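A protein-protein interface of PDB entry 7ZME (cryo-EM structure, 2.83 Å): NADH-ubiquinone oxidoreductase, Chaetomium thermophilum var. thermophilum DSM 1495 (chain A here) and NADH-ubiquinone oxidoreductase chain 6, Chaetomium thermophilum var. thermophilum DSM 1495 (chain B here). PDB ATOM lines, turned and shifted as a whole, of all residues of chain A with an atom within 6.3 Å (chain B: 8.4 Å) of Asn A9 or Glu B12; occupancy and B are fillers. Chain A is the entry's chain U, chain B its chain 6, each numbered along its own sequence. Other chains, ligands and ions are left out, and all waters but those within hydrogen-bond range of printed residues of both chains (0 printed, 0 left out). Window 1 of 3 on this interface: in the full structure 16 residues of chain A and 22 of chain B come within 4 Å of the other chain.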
ATOM      1  N   PRO A   6      25.476  11.285  29.998  1.00  0.00           N
ATOM      2  CA  PRO A   6      24.582  10.733  28.982  1.00  0.00           C
ATOM      3  C   PRO A   6      25.288  10.134  27.759  1.00  0.00           C
ATOM      4  O   PRO A   6      26.294  10.674  27.346  1.00  0.00           O
ATOM      5  CB  PRO A   6      23.774  11.965  28.556  1.00  0.00           C
ATOM      6  CG  PRO A   6      24.656  13.140  28.881  1.00  0.00           C
ATOM      7  CD  PRO A   6      25.329  12.730  30.168  1.00  0.00           C
ATOM      8  N   ALA A   7      24.752   9.044  27.207  1.00  0.00           N
ATOM      9  CA  ALA A   7      25.323   8.469  26.001  1.00  0.00           C
ATOM     10  C   ALA A   7      24.430   8.611  24.784  1.00  0.00           C
ATOM     11  O   ALA A   7      24.909   8.432  23.664  1.00  0.00           O
ATOM     12  CB  ALA A   7      25.638   6.980  26.212  1.00  0.00           C
ATOM     13  N   PHE A   8      23.150   8.930  24.972  1.00  0.00           N
ATOM     14  CA  PHE A   8      22.196   9.040  23.877  1.00  0.00           C
ATOM     15  C   PHE A   8      21.295  10.259  24.029  1.00  0.00           C
ATOM     16  O   PHE A   8      20.125  10.215  23.641  1.00  0.00           O
ATOM     17  CB  PHE A   8      21.360   7.764  23.774  1.00  0.00           C
ATOM     18  CG  PHE A   8      22.161   6.547  23.421  1.00  0.00           C
ATOM     19  CD1 PHE A   8      22.505   6.281  22.114  1.00  0.00           C
ATOM     20  CD2 PHE A   8      22.586   5.677  24.403  1.00  0.00           C
ATOM     21  CE1 PHE A   8      23.245   5.169  21.795  1.00  0.00           C
ATOM     22  CE2 PHE A   8      23.328   4.565  24.090  1.00  0.00           C
ATOM     23  CZ  PHE A   8      23.657   4.309  22.781  1.00  0.00           C
ATOM     24  N   ASN A   9      21.812  11.343  24.596  1.00  0.00           N
ATOM     25  CA  ASN A   9      21.017  12.547  24.783  1.00  0.00           C
ATOM     26  C   ASN A   9      20.827  13.262  23.450  1.00  0.00           C
ATOM     27  O   ASN A   9      21.791  13.494  22.716  1.00  0.00           O
ATOM     28  CB  ASN A   9      21.691  13.472  25.791  1.00  0.00           C
ATOM     29  CG  ASN A   9      23.143  13.738  25.455  1.00  0.00           C
ATOM     30  OD1 ASN A   9      23.926  12.811  25.266  1.00  0.00           O
ATOM     31  ND2 ASN A   9      23.509  15.007  25.380  1.00  0.00           N
ATOM     32  N   GLN A  10      19.582  13.603  23.137  1.00  0.00           N
ATOM     33  CA  GLN A  10      19.263  14.412  21.975  1.00  0.00           C
ATOM     34  C   GLN A  10      18.388  15.601  22.329  1.00  0.00           C
ATOM     35  O   GLN A  10      18.002  16.355  21.431  1.00  0.00           O
ATOM     36  CB  GLN A  10      18.556  13.571  20.902  1.00  0.00           C
ATOM     37  CG  GLN A  10      19.270  12.284  20.542  1.00  0.00           C
ATOM     38  CD  GLN A  10      20.338  12.493  19.491  1.00  0.00           C
ATOM     39  OE1 GLN A  10      21.518  12.257  19.734  1.00  0.00           O
ATOM     40  NE2 GLN A  10      19.925  12.942  18.311  1.00  0.00           N
ATOM     41  N   HIS A  11      18.077  15.773  23.609  1.00  0.00           N
ATOM     42  CA  HIS A  11      17.108  16.821  24.005  1.00  0.00           C
ATOM     43  C   HIS A  11      17.483  17.449  25.330  1.00  0.00           C
ATOM     44  O   HIS A  11      18.136  16.788  26.133  1.00  0.00           O
ATOM     45  CB  HIS A  11      15.700  16.227  24.147  1.00  0.00           C
ATOM     46  CG  HIS A  11      15.100  15.782  22.860  1.00  0.00           C
ATOM     47  ND1 HIS A  11      14.635  16.674  21.919  1.00  0.00           N
ATOM     48  CD2 HIS A  11      14.895  14.549  22.352  1.00  0.00           C
ATOM     49  CE1 HIS A  11      14.168  16.013  20.883  1.00  0.00           C
ATOM     50  NE2 HIS A  11      14.316  14.706  21.124  1.00  0.00           N
ATOM     51  N   VAL A  12      17.157  18.727  25.473  1.00  0.00           N
ATOM     52  CA  VAL A  12      17.417  19.452  26.743  1.00  0.00           C
ATOM     53  C   VAL A  12      16.061  19.853  27.334  1.00  0.00           C
ATOM     54  O   VAL A  12      15.198  20.293  26.563  1.00  0.00           O
ATOM     55  CB  VAL A  12      18.320  20.668  26.468  1.00  0.00           C
ATOM     56  CG1 VAL A  12      18.153  21.762  27.504  1.00  0.00           C
ATOM     57  CG2 VAL A  12      19.780  20.269  26.316  1.00  0.00           C
ATOM     58  N   LEU B   9      10.772  21.580  25.776  1.00  0.00           N
ATOM     59  CA  LEU B   9      11.627  20.527  25.186  1.00  0.00           C
ATOM     60  C   LEU B   9      12.401  21.185  24.052  1.00  0.00           C
ATOM     61  O   LEU B   9      11.853  22.080  23.404  1.00  0.00           O
ATOM     62  CB  LEU B   9      10.807  19.318  24.732  1.00  0.00           C
ATOM     63  CG  LEU B   9      11.598  18.025  24.544  1.00  0.00           C
ATOM     64  CD1 LEU B   9      12.432  17.713  25.775  1.00  0.00           C
ATOM     65  CD2 LEU B   9      10.664  16.868  24.229  1.00  0.00           C
ATOM     66  N   LEU B  10      13.641  20.781  23.862  1.00  0.00           N
ATOM     67  CA  LEU B  10      14.489  21.363  22.840  1.00  0.00           C
ATOM     68  C   LEU B  10      15.412  20.291  22.292  1.00  0.00           C
ATOM     69  O   LEU B  10      15.662  19.276  22.938  1.00  0.00           O
ATOM     70  CB  LEU B  10      15.290  22.535  23.416  1.00  0.00           C
ATOM     71  CG  LEU B  10      15.946  23.510  22.448  1.00  0.00           C
ATOM     72  CD1 LEU B  10      14.951  24.538  21.988  1.00  0.00           C
ATOM     73  CD2 LEU B  10      17.113  24.171  23.143  1.00  0.00           C
ATOM     74  N   LYS B  11      15.914  20.526  21.085  1.00  0.00           N
ATOM     75  CA  LYS B  11      16.898  19.644  20.477  1.00  0.00           C
ATOM     76  C   LYS B  11      18.296  20.138  20.816  1.00  0.00           C
ATOM     77  O   LYS B  11      18.577  21.335  20.720  1.00  0.00           O
ATOM     78  CB  LYS B  11      16.707  19.579  18.963  1.00  0.00           C
ATOM     79  CG  LYS B  11      15.442  18.856  18.529  1.00  0.00           C
ATOM     80  CD  LYS B  11      15.705  17.936  17.349  1.00  0.00           C
ATOM     81  CE  LYS B  11      14.474  17.112  17.008  1.00  0.00           C
ATOM     82  NZ  LYS B  11      14.613  16.423  15.697  1.00  0.00           N
ATOM     83  N   GLU B  12      19.163  19.216  21.216  1.00  0.00           N
ATOM     84  CA  GLU B  12      20.550  19.543  21.517  1.00  0.00           C
ATOM     85  C   GLU B  12      21.326  19.702  20.214  1.00  0.00           C
ATOM     86  O   GLU B  12      21.421  18.757  19.426  1.00  0.00           O
ATOM     87  CB  GLU B  12      21.161  18.451  22.391  1.00  0.00           C
ATOM     88  CG  GLU B  12      22.308  18.916  23.256  1.00  0.00           C
ATOM     89  CD  GLU B  12      22.666  17.908  24.324  1.00  0.00           C
ATOM     90  OE1 GLU B  12      23.701  18.092  24.996  1.00  0.00           O
ATOM     91  OE2 GLU B  12      21.909  16.930  24.492  1.00  0.00           O
ATOM     92  N   ILE B  13      21.886  20.891  19.990  1.00  0.00           N
ATOM     93  CA  ILE B  13      22.491  21.199  18.697  1.00  0.00           C
ATOM     94  C   ILE B  13      23.860  20.542  18.561  1.00  0.00           C
ATOM     95  O   ILE B  13      24.118  19.813  17.597  1.00  0.00           O
ATOM     96  CB  ILE B  13      22.553  22.725  18.481  1.00  0.00           C
ATOM     97  CG1 ILE B  13      23.216  23.053  17.140  1.00  0.00           C
ATOM     98  CG2 ILE B  13      23.221  23.443  19.657  1.00  0.00           C
ATOM     99  CD1 ILE B  13      23.053  24.494  16.714  1.00  0.00           C
ATOM    100  N   TYR B  14      24.756  20.790  19.504  1.00  0.00           N
ATOM    101  CA  TYR B  14      26.004  20.055  19.629  1.00  0.00           C
ATOM    102  C   TYR B  14      25.975  19.293  20.945  1.00  0.00           C
ATOM    103  O   TYR B  14      24.999  19.348  21.694  1.00  0.00           O
ATOM    104  CB  TYR B  14      27.218  20.987  19.561  1.00  0.00           C
ATOM    105  CG  TYR B  14      27.300  21.833  18.310  1.00  0.00           C
ATOM    106  CD1 TYR B  14      26.625  23.040  18.215  1.00  0.00           C
ATOM    107  CD2 TYR B  14      28.067  21.429  17.227  1.00  0.00           C
ATOM    108  CE1 TYR B  14      26.701  23.811  17.076  1.00  0.00           C
ATOM    109  CE2 TYR B  14      28.149  22.196  16.085  1.00  0.00           C
ATOM    110  CZ  TYR B  14      27.465  23.385  16.014  1.00  0.00           C
ATOM    111  OH  TYR B  14      27.550  24.151  14.875  1.00  0.00           O
ATOM    112  N   THR B  15      27.053  18.570  21.225  1.00  0.00           N
ATOM    113  CA  THR B  15      27.247  17.853  22.480  1.00  0.00           C
ATOM    114  C   THR B  15      26.181  16.787  22.724  1.00  0.00           C
ATOM    115  O   THR B  15      26.172  16.161  23.790  1.00  0.00           O
ATOM    116  CB  THR B  15      27.311  18.811  23.681  1.00  0.00           C
ATOM    117  OG1 THR B  15      26.077  19.529  23.801  1.00  0.00           O
ATOM    118  CG2 THR B  15      28.441  19.810  23.500  1.00  0.00           C
ATOM    119  N   ASN B  16      25.286  16.566  21.768  1.00  0.00           N
ATOM    120  CA  ASN B  16      24.326  15.484  21.873  1.00  0.00           C
ATOM    121  C   ASN B  16      25.018  14.135  21.700  1.00  0.00           C
ATOM    122  O   ASN B  16      26.111  14.031  21.137  1.00  0.00           O
ATOM    123  CB  ASN B  16      23.211  15.655  20.842  1.00  0.00           C
ATOM    124  CG  ASN B  16      23.730  15.766  19.427  1.00  0.00           C
ATOM    125  OD1 ASN B  16      24.929  15.667  19.179  1.00  0.00           O
ATOM    126  ND2 ASN B  16      22.822  15.969  18.485  1.00  0.00           N
ATOM    127  N   GLY B  17      24.367  13.095  22.199  1.00  0.00           N
ATOM    128  CA  GLY B  17      24.923  11.762  22.201  1.00  0.00           C
ATOM    129  C   GLY B  17      24.608  11.002  20.935  1.00  0.00           C
ATOM    130  O   GLY B  17      24.206  11.569  19.916  1.00  0.00           O
ATOM    131  N   SER B  18      24.803   9.692  21.006  1.00  0.00           N
ATOM    132  CA  SER B  18      24.506   8.814  19.889  1.00  0.00           C
ATOM    133  C   SER B  18      22.996   8.634  19.761  1.00  0.00           C
ATOM    134  O   SER B  18      22.208   9.171  20.544  1.00  0.00           O
ATOM    135  CB  SER B  18      25.215   7.475  20.074  1.00  0.00           C
ATOM    136  OG  SER B  18      24.966   6.604  18.987  1.00  0.00           O
ATOM    137  N   THR B  19      22.582   7.872  18.757  1.00  0.00           N
ATOM    138  CA  THR B  19      21.192   7.474  18.614  1.00  0.00           C
ATOM    139  C   THR B  19      21.011   6.075  19.184  1.00  0.00           C
ATOM    140  O   THR B  19      21.858   5.198  18.990  1.00  0.00           O
ATOM    141  CB  THR B  19      20.743   7.528  17.149  1.00  0.00           C
ATOM    142  OG1 THR B  19      19.332   7.292  17.066  1.00  0.00           O
ATOM    143  CG2 THR B  19      21.485   6.507  16.295  1.00  0.00           C
ATOM    144  N   HIS B  20      19.921   5.878  19.921  1.00  0.00           N
ATOM    145  CA  HIS B  20      19.655   4.574  20.510  1.00  0.00           C
ATOM    146  C   HIS B  20      19.010   3.617  19.523  1.00  0.00           C
ATOM    147  O   HIS B  20      18.717   2.474  19.891  1.00  0.00           O
ATOM    148  CB  HIS B  20      18.780   4.718  21.758  1.00  0.00           C
ATOM    149  CG  HIS B  20      17.417   5.268  21.482  1.00  0.00           C
ATOM    150  ND1 HIS B  20      17.188   6.605  21.245  1.00  0.00           N
ATOM    151  CD2 HIS B  20      16.210   4.659  21.401  1.00  0.00           C
ATOM    152  CE1 HIS B  20      15.900   6.799  21.031  1.00  0.00           C
ATOM    153  NE2 HIS B  20      15.284   5.633  21.120  1.00  0.00           N
ATOM    154  N   PHE B 169      14.845   9.607  30.511  1.00  0.00           N
ATOM    155  CA  PHE B 169      15.889   9.728  31.551  1.00  0.00           C
ATOM    156  C   PHE B 169      16.423  11.154  31.566  1.00  0.00           C
ATOM    157  O   PHE B 169      16.652  11.725  30.502  1.00  0.00           O
ATOM    158  CB  PHE B 169      16.963   8.668  31.330  1.00  0.00           C
ATOM    159  CG  PHE B 169      16.485   7.250  31.496  1.00  0.00           C
ATOM    160  CD1 PHE B 169      16.243   6.729  32.753  1.00  0.00           C
ATOM    161  CD2 PHE B 169      16.279   6.439  30.395  1.00  0.00           C
ATOM    162  CE1 PHE B 169      15.807   5.423  32.902  1.00  0.00           C
ATOM    163  CE2 PHE B 169      15.839   5.135  30.547  1.00  0.00           C
ATOM    164  CZ  PHE B 169      15.602   4.629  31.801  1.00  0.00           C
ATOM    165  N   THR B 171      19.424  13.813  33.098  1.00  0.00           N
ATOM    166  CA  THR B 171      20.722  13.923  33.747  1.00  0.00           C
ATOM    167  C   THR B 171      21.120  15.386  33.871  1.00  0.00           C
ATOM    168  O   THR B 171      20.817  16.208  33.005  1.00  0.00           O
ATOM    169  CB  THR B 171      21.830  13.165  32.997  1.00  0.00           C
ATOM    170  OG1 THR B 171      22.154  13.853  31.784  1.00  0.00           O
ATOM    171  CG2 THR B 171      21.403  11.746  32.678  1.00  0.00           C
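Of the 14 printed residues of chain B, 11 touch a printed residue of chain A.
Hydrophobic or aromatic side chains of chain A within 4 Å of the printed part of chain B: Pro A6, Phe A8 and His A11.
Among the printed residues, no Asp or Glu carboxylate lies within 4 Å of a Lys or Arg side-chain nitrogen of the other chain.
CD of Pro A6 touches OG1 of Thr B171 (3.7 Å).
Gly B17 touches Ala A7.
Phe A8 touches Ser B18 (CD1 to O, 3.3 Å).
Phe A8 touches Thr B19 (CE1 to O, 3.1 Å).
CD1 of Phe A8 touches N of His B20, 3.4 Å away.
O of Asn A9 touches CB of Asn B16, 3.2 Å away.
O of Gln A10 touches CA of Lys B11, at 3.6 Å.
Gln A10 touches Asn B16.
CB of His A11 touches CD1 of Leu B9, 3.9 Å away.
O of Val A12 touches CA of Leu B9 (3.8 Å).
Asn A9 touches just these residues of chain B: Glu B12 (2.7 Å), Thr B15 (3.3 Å), Asn B16 (3.2 Å) and Gly B17 (2.7 Å).
Of chain A, only Asn A9 (2.7 Å) and Gln A10 (3.1 Å) come within 4 Å of Glu B12.
Ile B13 touches none of the printed residues of chain A.
Of the printed residues of chain A, Thr B15 touches Asn A9 (3.3 Å).
Of the printed residues of chain A, Ser B18 touches Ala A7, Phe A8 and Gln A10.
Phe B169 touches none of the printed residues of chain A.
The nearest printed residue of chain A that does not touch Thr B171 is Asn A9 (6.0 Å).
The side-chain carboxylate (OE1) of Glu B12 sits at hydrogen-bond distance from the side-chain hydroxyl (OG1) of Thr B15, at 3.0 Å.
ND2 of Asn B16 lies within hydrogen-bond range of O of Glu B12.
The backbone NH (N) of Ser B18 sits at hydrogen-bond distance from the backbone carbonyl oxygen (O) of Ala A7.
The side-chain amide nitrogen (ND2) of Asn A9 sits at hydrogen-bond distance from the side-chain carboxylate (OE2) of Glu B12 (2.7 Å).
The backbone carbonyl oxygen of Thr B15 sits at hydrogen-bond distance from the side-chain amide nitrogen of Asn A9 (3.3 Å).
N of Gly B17 lies within hydrogen-bond range of O of Asn A9 (2.7 Å).
The backbone NH of Glu B12 sits at hydrogen-bond distance from the backbone carbonyl oxygen of Gln A10, 3.1 Å away.
OE1 of Gln A10 lies close to O of Gly B17, 2.8 Å away.
The side-chain amide oxygen (OE1) of Gln A10 sits close to the backbone carbonyl oxygen (O) of Ser B18.
The backbone carbonyl oxygen of Leu B10 is in hydrogen-bond range of a ring nitrogen (ND1) of His A11.
N of Val A12 sits at hydrogen-bond distance from O of Leu B10 (3.0 Å).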
